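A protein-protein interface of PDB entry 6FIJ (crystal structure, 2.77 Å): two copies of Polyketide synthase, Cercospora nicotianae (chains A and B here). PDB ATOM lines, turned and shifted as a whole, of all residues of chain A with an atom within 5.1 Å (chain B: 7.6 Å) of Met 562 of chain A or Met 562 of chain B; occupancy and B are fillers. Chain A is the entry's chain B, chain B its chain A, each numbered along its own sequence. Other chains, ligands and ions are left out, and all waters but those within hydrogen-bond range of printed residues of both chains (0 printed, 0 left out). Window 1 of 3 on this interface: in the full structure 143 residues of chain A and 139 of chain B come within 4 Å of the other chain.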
ATOM      1  N   TRP A 502       5.299 -25.565  -3.254  1.00  0.00           N
ATOM      2  CA  TRP A 502       3.863 -25.438  -3.052  1.00  0.00           C
ATOM      3  C   TRP A 502       3.151 -25.625  -4.384  1.00  0.00           C
ATOM      4  O   TRP A 502       3.571 -25.065  -5.401  1.00  0.00           O
ATOM      5  CB  TRP A 502       3.491 -24.067  -2.469  1.00  0.00           C
ATOM      6  CG  TRP A 502       3.967 -23.827  -1.068  1.00  0.00           C
ATOM      7  CD1 TRP A 502       3.233 -23.932   0.076  1.00  0.00           C
ATOM      8  CD2 TRP A 502       5.281 -23.422  -0.666  1.00  0.00           C
ATOM      9  NE1 TRP A 502       4.008 -23.624   1.167  1.00  0.00           N
ATOM     10  CE2 TRP A 502       5.270 -23.308   0.739  1.00  0.00           C
ATOM     11  CE3 TRP A 502       6.467 -23.148  -1.354  1.00  0.00           C
ATOM     12  CZ2 TRP A 502       6.398 -22.934   1.467  1.00  0.00           C
ATOM     13  CZ3 TRP A 502       7.586 -22.777  -0.629  1.00  0.00           C
ATOM     14  CH2 TRP A 502       7.543 -22.672   0.765  1.00  0.00           C
ATOM     15  N   TYR A 547       3.994 -28.839   0.184  1.00  0.00           N
ATOM     16  CA  TYR A 547       2.567 -28.708   0.461  1.00  0.00           C
ATOM     17  C   TYR A 547       1.750 -28.750  -0.824  1.00  0.00           C
ATOM     18  O   TYR A 547       2.208 -28.332  -1.890  1.00  0.00           O
ATOM     19  CB  TYR A 547       2.247 -27.392   1.186  1.00  0.00           C
ATOM     20  CG  TYR A 547       2.762 -27.299   2.604  1.00  0.00           C
ATOM     21  CD1 TYR A 547       2.034 -27.821   3.661  1.00  0.00           C
ATOM     22  CD2 TYR A 547       3.966 -26.671   2.886  1.00  0.00           C
ATOM     23  CE1 TYR A 547       2.497 -27.728   4.958  1.00  0.00           C
ATOM     24  CE2 TYR A 547       4.432 -26.575   4.182  1.00  0.00           C
ATOM     25  CZ  TYR A 547       3.694 -27.108   5.212  1.00  0.00           C
ATOM     26  OH  TYR A 547       4.151 -27.020   6.507  1.00  0.00           O
ATOM     27  N   ILE A 549      -2.237 -27.422  -1.848  1.00  0.00           N
ATOM     28  CA  ILE A 549      -3.361 -26.610  -1.394  1.00  0.00           C
ATOM     29  C   ILE A 549      -4.552 -26.889  -2.297  1.00  0.00           C
ATOM     30  O   ILE A 549      -4.413 -26.925  -3.525  1.00  0.00           O
ATOM     31  CB  ILE A 549      -3.018 -25.110  -1.404  1.00  0.00           C
ATOM     32  CG1 ILE A 549      -1.715 -24.841  -0.645  1.00  0.00           C
ATOM     33  CG2 ILE A 549      -4.168 -24.297  -0.819  1.00  0.00           C
ATOM     34  CD1 ILE A 549      -1.772 -25.186   0.826  1.00  0.00           C
ATOM     35  N   ALA A 558      -3.848 -19.377  -3.853  1.00  0.00           N
ATOM     36  CA  ALA A 558      -3.752 -19.707  -2.436  1.00  0.00           C
ATOM     37  C   ALA A 558      -2.386 -20.294  -2.114  1.00  0.00           C
ATOM     38  O   ALA A 558      -1.785 -19.961  -1.086  1.00  0.00           O
ATOM     39  CB  ALA A 558      -4.864 -20.680  -2.047  1.00  0.00           C
ATOM     40  N   ALA A 559      -1.876 -21.164  -2.988  1.00  0.00           N
ATOM     41  CA  ALA A 559      -0.541 -21.718  -2.791  1.00  0.00           C
ATOM     42  C   ALA A 559       0.520 -20.636  -2.916  1.00  0.00           C
ATOM     43  O   ALA A 559       1.469 -20.593  -2.125  1.00  0.00           O
ATOM     44  CB  ALA A 559      -0.286 -22.835  -3.800  1.00  0.00           C
ATOM     45  N   LEU A 560       0.379 -19.752  -3.904  1.00  0.00           N
ATOM     46  CA  LEU A 560       1.287 -18.617  -4.011  1.00  0.00           C
ATOM     47  C   LEU A 560       1.270 -17.785  -2.734  1.00  0.00           C
ATOM     48  O   LEU A 560       2.308 -17.265  -2.309  1.00  0.00           O
ATOM     49  CB  LEU A 560       0.909 -17.765  -5.225  1.00  0.00           C
ATOM     50  CG  LEU A 560       1.733 -16.500  -5.482  1.00  0.00           C
ATOM     51  CD1 LEU A 560       3.213 -16.815  -5.556  1.00  0.00           C
ATOM     52  CD2 LEU A 560       1.275 -15.814  -6.760  1.00  0.00           C
ATOM     53  N   HIS A 561       0.101 -17.662  -2.100  1.00  0.00           N
ATOM     54  CA  HIS A 561       0.000 -16.899  -0.859  1.00  0.00           C
ATOM     55  C   HIS A 561       0.790 -17.562   0.262  1.00  0.00           C
ATOM     56  O   HIS A 561       1.554 -16.898   0.974  1.00  0.00           O
ATOM     57  CB  HIS A 561      -1.470 -16.744  -0.466  1.00  0.00           C
ATOM     58  CG  HIS A 561      -1.694 -15.827   0.696  1.00  0.00           C
ATOM     59  ND1 HIS A 561      -2.919 -15.697   1.314  1.00  0.00           N
ATOM     60  CD2 HIS A 561      -0.852 -14.991   1.349  1.00  0.00           C
ATOM     61  CE1 HIS A 561      -2.822 -14.822   2.299  1.00  0.00           C
ATOM     62  NE2 HIS A 561      -1.578 -14.379   2.341  1.00  0.00           N
ATOM     63  N   MET A 562       0.613 -18.874   0.441  1.00  0.00           N
ATOM     64  CA  MET A 562       1.347 -19.582   1.485  1.00  0.00           C
ATOM     65  C   MET A 562       2.849 -19.483   1.258  1.00  0.00           C
ATOM     66  O   MET A 562       3.617 -19.290   2.208  1.00  0.00           O
ATOM     67  CB  MET A 562       0.912 -21.047   1.536  1.00  0.00           C
ATOM     68  CG  MET A 562      -0.583 -21.272   1.725  1.00  0.00           C
ATOM     69  SD  MET A 562      -1.108 -21.226   3.452  1.00  0.00           S
ATOM     70  CE  MET A 562      -1.385 -19.474   3.721  1.00  0.00           C
ATOM     71  N   ALA A 563       3.284 -19.612   0.003  1.00  0.00           N
ATOM     72  CA  ALA A 563       4.708 -19.544  -0.299  1.00  0.00           C
ATOM     73  C   ALA A 563       5.274 -18.167   0.026  1.00  0.00           C
ATOM     74  O   ALA A 563       6.382 -18.054   0.564  1.00  0.00           O
ATOM     75  CB  ALA A 563       4.945 -19.889  -1.767  1.00  0.00           C
ATOM     76  N   CYS A 564       4.531 -17.107  -0.296  1.00  0.00           N
ATOM     77  CA  CYS A 564       5.007 -15.762   0.004  1.00  0.00           C
ATOM     78  C   CYS A 564       5.130 -15.544   1.507  1.00  0.00           C
ATOM     79  O   CYS A 564       6.062 -14.876   1.970  1.00  0.00           O
ATOM     80  CB  CYS A 564       4.079 -14.722  -0.623  1.00  0.00           C
ATOM     81  SG  CYS A 564       4.250 -14.580  -2.419  1.00  0.00           S
ATOM     82  N   ASN A 565       4.204 -16.106   2.289  1.00  0.00           N
ATOM     83  CA  ASN A 565       4.307 -15.996   3.741  1.00  0.00           C
ATOM     84  C   ASN A 565       5.566 -16.681   4.254  1.00  0.00           C
ATOM     85  O   ASN A 565       6.252 -16.153   5.136  1.00  0.00           O
ATOM     86  CB  ASN A 565       3.068 -16.591   4.410  1.00  0.00           C
ATOM     87  CG  ASN A 565       1.854 -15.687   4.300  1.00  0.00           C
ATOM     88  OD1 ASN A 565       1.979 -14.479   4.103  1.00  0.00           O
ATOM     89  ND2 ASN A 565       0.668 -16.270   4.442  1.00  0.00           N
ATOM     90  N   ALA A 566       5.888 -17.858   3.712  1.00  0.00           N
ATOM     91  CA  ALA A 566       7.104 -18.557   4.116  1.00  0.00           C
ATOM     92  C   ALA A 566       8.336 -17.706   3.837  1.00  0.00           C
ATOM     93  O   ALA A 566       9.214 -17.556   4.694  1.00  0.00           O
ATOM     94  CB  ALA A 566       7.198 -19.900   3.394  1.00  0.00           C
ATOM     95  N   ARG A 569       8.474 -14.789   6.294  1.00  0.00           N
ATOM     96  CA  ARG A 569       8.849 -15.165   7.650  1.00  0.00           C
ATOM     97  C   ARG A 569      10.218 -15.829   7.721  1.00  0.00           C
ATOM     98  O   ARG A 569      10.667 -16.170   8.820  1.00  0.00           O
ATOM     99  CB  ARG A 569       7.790 -16.090   8.266  1.00  0.00           C
ATOM    100  CG  ARG A 569       7.777 -17.509   7.724  1.00  0.00           C
ATOM    101  CD  ARG A 569       6.834 -18.391   8.528  1.00  0.00           C
ATOM    102  NE  ARG A 569       6.766 -19.749   7.992  1.00  0.00           N
ATOM    103  CZ  ARG A 569       5.910 -20.148   7.057  1.00  0.00           C
ATOM    104  NH1 ARG A 569       5.032 -19.299   6.537  1.00  0.00           N
ATOM    105  NH2 ARG A 569       5.932 -21.406   6.636  1.00  0.00           N
ATOM    106  N   TRP B 502      -8.783 -24.171   8.617  1.00  0.00           N
ATOM    107  CA  TRP B 502      -7.813 -25.022   7.940  1.00  0.00           C
ATOM    108  C   TRP B 502      -8.178 -26.474   8.206  1.00  0.00           C
ATOM    109  O   TRP B 502      -8.468 -26.844   9.348  1.00  0.00           O
ATOM    110  CB  TRP B 502      -6.380 -24.760   8.428  1.00  0.00           C
ATOM    111  CG  TRP B 502      -5.798 -23.432   8.041  1.00  0.00           C
ATOM    112  CD1 TRP B 502      -4.923 -23.192   7.021  1.00  0.00           C
ATOM    113  CD2 TRP B 502      -6.030 -22.168   8.677  1.00  0.00           C
ATOM    114  NE1 TRP B 502      -4.600 -21.856   6.980  1.00  0.00           N
ATOM    115  CE2 TRP B 502      -5.266 -21.207   7.984  1.00  0.00           C
ATOM    116  CE3 TRP B 502      -6.809 -21.756   9.760  1.00  0.00           C
ATOM    117  CZ2 TRP B 502      -5.263 -19.860   8.339  1.00  0.00           C
ATOM    118  CZ3 TRP B 502      -6.803 -20.417  10.110  1.00  0.00           C
ATOM    119  CH2 TRP B 502      -6.035 -19.486   9.402  1.00  0.00           C
ATOM    120  N   PRO B 545      -9.652 -16.508   6.199  1.00  0.00           N
ATOM    121  CA  PRO B 545      -9.186 -17.464   5.189  1.00  0.00           C
ATOM    122  C   PRO B 545      -9.758 -18.859   5.405  1.00  0.00           C
ATOM    123  O   PRO B 545     -10.164 -19.239   6.504  1.00  0.00           O
ATOM    124  CB  PRO B 545      -7.663 -17.455   5.364  1.00  0.00           C
ATOM    125  CG  PRO B 545      -7.426 -16.913   6.727  1.00  0.00           C
ATOM    126  CD  PRO B 545      -8.547 -15.969   7.008  1.00  0.00           C
ATOM    127  N   TYR B 547      -8.842 -22.880   3.994  1.00  0.00           N
ATOM    128  CA  TYR B 547      -7.832 -23.665   3.296  1.00  0.00           C
ATOM    129  C   TYR B 547      -8.019 -25.150   3.567  1.00  0.00           C
ATOM    130  O   TYR B 547      -8.479 -25.551   4.639  1.00  0.00           O
ATOM    131  CB  TYR B 547      -6.409 -23.282   3.726  1.00  0.00           C
ATOM    132  CG  TYR B 547      -5.946 -21.912   3.291  1.00  0.00           C
ATOM    133  CD1 TYR B 547      -5.405 -21.711   2.031  1.00  0.00           C
ATOM    134  CD2 TYR B 547      -6.016 -20.827   4.154  1.00  0.00           C
ATOM    135  CE1 TYR B 547      -4.966 -20.463   1.633  1.00  0.00           C
ATOM    136  CE2 TYR B 547      -5.577 -19.577   3.763  1.00  0.00           C
ATOM    137  CZ  TYR B 547      -5.053 -19.400   2.503  1.00  0.00           C
ATOM    138  OH  TYR B 547      -4.616 -18.154   2.109  1.00  0.00           O
ATOM    139  N   THR B 548      -7.632 -25.959   2.581  1.00  0.00           N
ATOM    140  CA  THR B 548      -7.478 -27.399   2.740  1.00  0.00           C
ATOM    141  C   THR B 548      -6.053 -27.783   2.363  1.00  0.00           C
ATOM    142  O   THR B 548      -5.536 -27.332   1.335  1.00  0.00           O
ATOM    143  CB  THR B 548      -8.485 -28.168   1.881  1.00  0.00           C
ATOM    144  OG1 THR B 548      -9.803 -27.979   2.410  1.00  0.00           O
ATOM    145  CG2 THR B 548      -8.161 -29.662   1.856  1.00  0.00           C
ATOM    146  N   ILE B 549      -5.424 -28.614   3.192  1.00  0.00           N
ATOM    147  CA  ILE B 549      -4.035 -29.023   3.013  1.00  0.00           C
ATOM    148  C   ILE B 549      -4.001 -30.515   2.711  1.00  0.00           C
ATOM    149  O   ILE B 549      -4.675 -31.305   3.382  1.00  0.00           O
ATOM    150  CB  ILE B 549      -3.189 -28.705   4.259  1.00  0.00           C
ATOM    151  CG1 ILE B 549      -3.379 -27.244   4.686  1.00  0.00           C
ATOM    152  CG2 ILE B 549      -1.715 -29.013   3.999  1.00  0.00           C
ATOM    153  CD1 ILE B 549      -2.915 -26.227   3.663  1.00  0.00           C
ATOM    154  N   SER B 555      -1.376 -34.436   6.703  1.00  0.00           N
ATOM    155  CA  SER B 555      -2.139 -33.266   6.284  1.00  0.00           C
ATOM    156  C   SER B 555      -2.591 -32.433   7.476  1.00  0.00           C
ATOM    157  O   SER B 555      -2.436 -31.207   7.482  1.00  0.00           O
ATOM    158  CB  SER B 555      -3.346 -33.710   5.456  1.00  0.00           C
ATOM    159  OG  SER B 555      -2.932 -34.357   4.267  1.00  0.00           O
ATOM    160  N   SER B 556      -3.153 -33.077   8.500  1.00  0.00           N
ATOM    161  CA  SER B 556      -3.757 -32.319   9.593  1.00  0.00           C
ATOM    162  C   SER B 556      -2.705 -31.534  10.373  1.00  0.00           C
ATOM    163  O   SER B 556      -2.898 -30.351  10.673  1.00  0.00           O
ATOM    164  CB  SER B 556      -4.539 -33.251  10.517  1.00  0.00           C
ATOM    165  OG  SER B 556      -3.717 -34.281  11.034  1.00  0.00           O
ATOM    166  N   LEU B 557      -1.578 -32.168  10.706  1.00  0.00           N
ATOM    167  CA  LEU B 557      -0.528 -31.431  11.402  1.00  0.00           C
ATOM    168  C   LEU B 557       0.104 -30.387  10.491  1.00  0.00           C
ATOM    169  O   LEU B 557       0.554 -29.339  10.967  1.00  0.00           O
ATOM    170  CB  LEU B 557       0.535 -32.386  11.947  1.00  0.00           C
ATOM    171  CG  LEU B 557       1.070 -31.992  13.329  1.00  0.00           C
ATOM    172  CD1 LEU B 557       0.017 -32.223  14.405  1.00  0.00           C
ATOM    173  CD2 LEU B 557       2.341 -32.747  13.671  1.00  0.00           C
ATOM    174  N   ALA B 558       0.147 -30.657   9.183  1.00  0.00           N
ATOM    175  CA  ALA B 558       0.572 -29.639   8.230  1.00  0.00           C
ATOM    176  C   ALA B 558      -0.379 -28.449   8.242  1.00  0.00           C
ATOM    177  O   ALA B 558       0.056 -27.294   8.187  1.00  0.00           O
ATOM    178  CB  ALA B 558       0.655 -30.243   6.828  1.00  0.00           C
ATOM    179  N   ALA B 559      -1.687 -28.712   8.311  1.00  0.00           N
ATOM    180  CA  ALA B 559      -2.655 -27.626   8.405  1.00  0.00           C
ATOM    181  C   ALA B 559      -2.512 -26.883   9.726  1.00  0.00           C
ATOM    182  O   ALA B 559      -2.597 -25.650   9.764  1.00  0.00           O
ATOM    183  CB  ALA B 559      -4.072 -28.170   8.248  1.00  0.00           C
ATOM    184  N   LEU B 560      -2.303 -27.618  10.819  1.00  0.00           N
ATOM    185  CA  LEU B 560      -2.044 -26.973  12.101  1.00  0.00           C
ATOM    186  C   LEU B 560      -0.845 -26.039  12.002  1.00  0.00           C
ATOM    187  O   LEU B 560      -0.823 -24.973  12.627  1.00  0.00           O
ATOM    188  CB  LEU B 560      -1.824 -28.036  13.179  1.00  0.00           C
ATOM    189  CG  LEU B 560      -1.515 -27.554  14.596  1.00  0.00           C
ATOM    190  CD1 LEU B 560      -2.569 -26.582  15.085  1.00  0.00           C
ATOM    191  CD2 LEU B 560      -1.419 -28.743  15.536  1.00  0.00           C
ATOM    192  N   HIS B 561       0.158 -26.420  11.210  1.00  0.00           N
ATOM    193  CA  HIS B 561       1.317 -25.557  11.002  1.00  0.00           C
ATOM    194  C   HIS B 561       0.909 -24.274  10.288  1.00  0.00           C
ATOM    195  O   HIS B 561       1.278 -23.170  10.704  1.00  0.00           O
ATOM    196  CB  HIS B 561       2.382 -26.317  10.206  1.00  0.00           C
ATOM    197  CG  HIS B 561       3.682 -25.589  10.071  1.00  0.00           C
ATOM    198  ND1 HIS B 561       4.401 -25.134  11.155  1.00  0.00           N
ATOM    199  CD2 HIS B 561       4.402 -25.250   8.975  1.00  0.00           C
ATOM    200  CE1 HIS B 561       5.503 -24.539  10.734  1.00  0.00           C
ATOM    201  NE2 HIS B 561       5.527 -24.594   9.414  1.00  0.00           N
ATOM    202  N   MET B 562       0.129 -24.404   9.211  1.00  0.00           N
ATOM    203  CA  MET B 562      -0.332 -23.230   8.477  1.00  0.00           C
ATOM    204  C   MET B 562      -1.159 -22.315   9.373  1.00  0.00           C
ATOM    205  O   MET B 562      -1.016 -21.088   9.324  1.00  0.00           O
ATOM    206  CB  MET B 562      -1.158 -23.665   7.266  1.00  0.00           C
ATOM    207  CG  MET B 562      -0.471 -24.644   6.318  1.00  0.00           C
ATOM    208  SD  MET B 562       0.579 -23.866   5.077  1.00  0.00           S
ATOM    209  CE  MET B 562       2.133 -23.698   5.963  1.00  0.00           C
ATOM    210  N   ALA B 563      -2.032 -22.897  10.198  1.00  0.00           N
ATOM    211  CA  ALA B 563      -2.874 -22.092  11.076  1.00  0.00           C
ATOM    212  C   ALA B 563      -2.039 -21.327  12.091  1.00  0.00           C
ATOM    213  O   ALA B 563      -2.299 -20.150  12.362  1.00  0.00           O
ATOM    214  CB  ALA B 563      -3.882 -22.986  11.795  1.00  0.00           C
ATOM    215  N   CYS B 564      -1.026 -21.980  12.663  1.00  0.00           N
ATOM    216  CA  CYS B 564      -0.186 -21.317  13.650  1.00  0.00           C
ATOM    217  C   CYS B 564       0.577 -20.156  13.026  1.00  0.00           C
ATOM    218  O   CYS B 564       0.766 -19.112  13.663  1.00  0.00           O
ATOM    219  CB  CYS B 564       0.776 -22.326  14.273  1.00  0.00           C
ATOM    220  SG  CYS B 564      -0.021 -23.488  15.402  1.00  0.00           S
ATOM    221  N   ASN B 565       1.022 -20.316  11.779  1.00  0.00           N
ATOM    222  CA  ASN B 565       1.700 -19.221  11.094  1.00  0.00           C
ATOM    223  C   ASN B 565       0.764 -18.033  10.902  1.00  0.00           C
ATOM    224  O   ASN B 565       1.174 -16.878  11.066  1.00  0.00           O
ATOM    225  CB  ASN B 565       2.251 -19.702   9.753  1.00  0.00           C
ATOM    226  CG  ASN B 565       3.492 -20.565   9.911  1.00  0.00           C
ATOM    227  OD1 ASN B 565       4.189 -20.492  10.926  1.00  0.00           O
ATOM    228  ND2 ASN B 565       3.775 -21.385   8.906  1.00  0.00           N
ATOM    229  N   ALA B 566      -0.495 -18.295  10.549  1.00  0.00           N
ATOM    230  CA  ALA B 566      -1.462 -17.213  10.398  1.00  0.00           C
ATOM    231  C   ALA B 566      -1.630 -16.446  11.703  1.00  0.00           C
ATOM    232  O   ALA B 566      -1.593 -15.211  11.722  1.00  0.00           O
ATOM    233  CB  ALA B 566      -2.804 -17.773   9.924  1.00  0.00           C
ATOM    234  N   LEU B 567      -1.814 -17.166  12.813  1.00  0.00           N
ATOM    235  CA  LEU B 567      -1.932 -16.507  14.108  1.00  0.00           C
ATOM    236  C   LEU B 567      -0.673 -15.716  14.445  1.00  0.00           C
ATOM    237  O   LEU B 567      -0.757 -14.576  14.916  1.00  0.00           O
ATOM    238  CB  LEU B 567      -2.218 -17.538  15.198  1.00  0.00           C
ATOM    239  CG  LEU B 567      -3.640 -18.093  15.255  1.00  0.00           C
ATOM    240  CD1 LEU B 567      -3.680 -19.359  16.093  1.00  0.00           C
ATOM    241  CD2 LEU B 567      -4.586 -17.048  15.821  1.00  0.00           C
ATOM    242  N   TRP B 568       0.502 -16.304  14.207  1.00  0.00           N
ATOM    243  CA  TRP B 568       1.750 -15.612  14.517  1.00  0.00           C
ATOM    244  C   TRP B 568       1.943 -14.400  13.617  1.00  0.00           C
ATOM    245  O   TRP B 568       2.450 -13.363  14.061  1.00  0.00           O
ATOM    246  CB  TRP B 568       2.928 -16.578  14.378  1.00  0.00           C
ATOM    247  CG  TRP B 568       3.084 -17.521  15.535  1.00  0.00           C
ATOM    248  CD1 TRP B 568       2.893 -17.240  16.856  1.00  0.00           C
ATOM    249  CD2 TRP B 568       3.454 -18.903  15.470  1.00  0.00           C
ATOM    250  NE1 TRP B 568       3.126 -18.357  17.617  1.00  0.00           N
ATOM    251  CE2 TRP B 568       3.470 -19.393  16.790  1.00  0.00           C
ATOM    252  CE3 TRP B 568       3.773 -19.773  14.423  1.00  0.00           C
ATOM    253  CZ2 TRP B 568       3.793 -20.712  17.091  1.00  0.00           C
ATOM    254  CZ3 TRP B 568       4.093 -21.081  14.724  1.00  0.00           C
ATOM    255  CH2 TRP B 568       4.100 -21.539  16.048  1.00  0.00           C
ATOM    256  N   GLU B 571      -2.772 -12.645  10.710  1.00  0.00           N
ATOM    257  CA  GLU B 571      -3.851 -12.622   9.727  1.00  0.00           C
ATOM    258  C   GLU B 571      -5.188 -12.974  10.360  1.00  0.00           C
ATOM    259  O   GLU B 571      -6.239 -12.559   9.858  1.00  0.00           O
ATOM    260  CB  GLU B 571      -3.548 -13.583   8.577  1.00  0.00           C
ATOM    261  CG  GLU B 571      -2.513 -13.064   7.593  1.00  0.00           C
ATOM    262  CD  GLU B 571      -2.191 -14.065   6.498  1.00  0.00           C
ATOM    263  OE1 GLU B 571      -2.895 -15.095   6.403  1.00  0.00           O
ATOM    264  OE2 GLU B 571      -1.234 -13.819   5.733  1.00  0.00           O
ATOM    265  N   VAL B 572      -5.173 -13.739  11.451  1.00  0.00           N
ATOM    266  CA  VAL B 572      -6.386 -14.114  12.162  1.00  0.00           C
ATOM    267  C   VAL B 572      -6.114 -14.076  13.659  1.00  0.00           C
ATOM    268  O   VAL B 572      -4.972 -14.164  14.112  1.00  0.00           O
ATOM    269  CB  VAL B 572      -6.890 -15.512  11.743  1.00  0.00           C
ATOM    270  CG1 VAL B 572      -7.347 -15.499  10.291  1.00  0.00           C
ATOM    271  CG2 VAL B 572      -5.800 -16.557  11.951  1.00  0.00           C
ATOM    272  N   ALA B 575      -8.490 -19.463  15.122  1.00  0.00           N
ATOM    273  CA  ALA B 575      -8.252 -20.434  14.065  1.00  0.00           C
ATOM    274  C   ALA B 575      -9.014 -21.715  14.352  1.00  0.00           C
ATOM    275  O   ALA B 575      -9.030 -22.201  15.487  1.00  0.00           O
ATOM    276  CB  ALA B 575      -6.758 -20.745  13.914  1.00  0.00           C
ATOM    277  N   VAL B 577      -8.919 -25.539  13.205  1.00  0.00           N
ATOM    278  CA  VAL B 577      -8.015 -26.506  12.594  1.00  0.00           C
ATOM    279  C   VAL B 577      -8.611 -27.895  12.762  1.00  0.00           C
ATOM    280  O   VAL B 577      -9.103 -28.241  13.840  1.00  0.00           O
ATOM    281  CB  VAL B 577      -6.608 -26.442  13.225  1.00  0.00           C
ATOM    282  CG1 VAL B 577      -5.690 -27.491  12.607  1.00  0.00           C
ATOM    283  CG2 VAL B 577      -6.017 -25.055  13.062  1.00  0.00           C
ATOM    284  N   ILE B 645       6.364 -25.530  16.112  1.00  0.00           N
ATOM    285  CA  ILE B 645       6.009 -26.524  15.109  1.00  0.00           C
ATOM    286  C   ILE B 645       6.796 -26.217  13.844  1.00  0.00           C
ATOM    287  O   ILE B 645       6.905 -25.056  13.435  1.00  0.00           O
ATOM    288  CB  ILE B 645       4.490 -26.544  14.849  1.00  0.00           C
ATOM    289  CG1 ILE B 645       4.157 -27.474  13.680  1.00  0.00           C
ATOM    290  CG2 ILE B 645       3.963 -25.136  14.592  1.00  0.00           C
ATOM    291  CD1 ILE B 645       2.679 -27.773  13.548  1.00  0.00           C
ATOM    292  N   THR B 647       8.535 -28.007   9.865  1.00  0.00           N
ATOM    293  CA  THR B 647       8.343 -28.950   8.773  1.00  0.00           C
ATOM    294  C   THR B 647       9.583 -28.961   7.895  1.00  0.00           C
ATOM    295  O   THR B 647      10.133 -27.904   7.574  1.00  0.00           O
ATOM    296  CB  THR B 647       7.116 -28.581   7.929  1.00  0.00           C
ATOM    297  OG1 THR B 647       5.929 -28.724   8.720  1.00  0.00           O
ATOM    298  CG2 THR B 647       7.011 -29.471   6.690  1.00  0.00           C
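The side-chain hydroxyl (OH) of Tyr 547 of chain B sits at hydrogen-bond distance from a ring nitrogen (ND1) of His 561 of chain A (3.1 Å).
The guanidinium group (NH2) of Arg 569 of chain A lies close to the side-chain amide nitrogen (ND2) of Asn 565 of chain B, at 3.1 Å.
OE2 of Glu 571 of chain B lies within hydrogen-bond range of NE2 of His 561 of chain A.
The side-chain carboxylate (OE2) of Glu 571 of chain B sits at hydrogen-bond distance from the side-chain amide nitrogen (ND2) of Asn 565 of chain A.
OG1 of Thr 647 of chain B is in hydrogen-bond range of OH of Tyr 547 of chain A.
SD of Met 562 of chain A sits close to SD of Met 562 of chain B.
A ring nitrogen (ND1) of His 561 of chain B lies close to the backbone carbonyl oxygen of Ile 645 of chain B (3.4 Å).
The backbone NH of Glu 571 of chain B sits at hydrogen-bond distance from the backbone carbonyl oxygen of Ala 566 of chain B, at 3.0 Å.
Among the printed residues, merely in contact across the chains: Tyr 547 of chain A with His 561 of chain B, Ile 549 of chain A with Ile 549 of chain B, Ile 549 of chain A with Thr 548 of chain B, Tyr 547 of chain A with Ala 558 of chain B, Ala 558 of chain A with Tyr 547 of chain B, Tyr 547 of chain A with Met 562 of chain B, Met 562 of chain A with Tyr 547 of chain B and Tyr 547 of chain A with Ile 549 of chain B.
Printed residues of chain B within 4 Å of Ile 549 of chain A: Thr 548 (3.6 Å) and Ile 549 (3.2 Å).
Printed residues of chain B within 4 Å of Ala 558 of chain A: Tyr 547.
Of chain B, only Tyr 547 and Met 562 come within 4 Å of Met 562 of chain A.
Printed residues of chain B within 4 Å of Asn 565 of chain A: Glu 571.
Of chain A, only Tyr 547 and Met 562 come within 4 Å of Met 562 of chain B.
The nearest residue of chain B that does not touch Met 562 of chain A is Trp 502 of chain B (5.0 Å).
The nearest printed residue of chain A that does not touch Met 562 of chain B is Arg 569 of chain A (4.5 Å).
The nearest printed residue of chain A that does not touch Thr 548 of chain B is Ala 558 of chain A (7.5 Å).
Of the 13 printed residues of chain A, 7 touch a printed residue of chain B.
Hydrophobic or aromatic side chains of chain A that line the printed part of chain B: Tyr 547, Ile 549, Ala 558, His 561 and Met 562.
Of the 25 printed residues of chain B, 9 touch a printed residue of chain A.
Along chain B the printed residues that touch a printed residue of chain A span positions 547 to 647.
Among the printed residues, 14 pairs touch across the chains.
Among the printed residues, no Asp or Glu carboxylate lies within 4 Å of a Lys or Arg side-chain nitrogen of the other chain.
Tyr 547 of chain A touches His 561 of chain B, and with the chains exchanged His 561 of chain A touches Tyr 547 of chain B.
Tyr 547 of chain A touches Met 562 of chain B, and with the chains exchanged Met 562 of chain A touches Tyr 547 of chain B.
Ile 549 of chain A touches its own counterpart, Ile 549 of chain B.
Met 562 of chain A touches its own counterpart, Met 562 of chain B.
12 positions are printed for both chains.
Of the 14 pairs that touch across the chains among the printed residues, 8 have their exchanged pair printed and touching as well.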
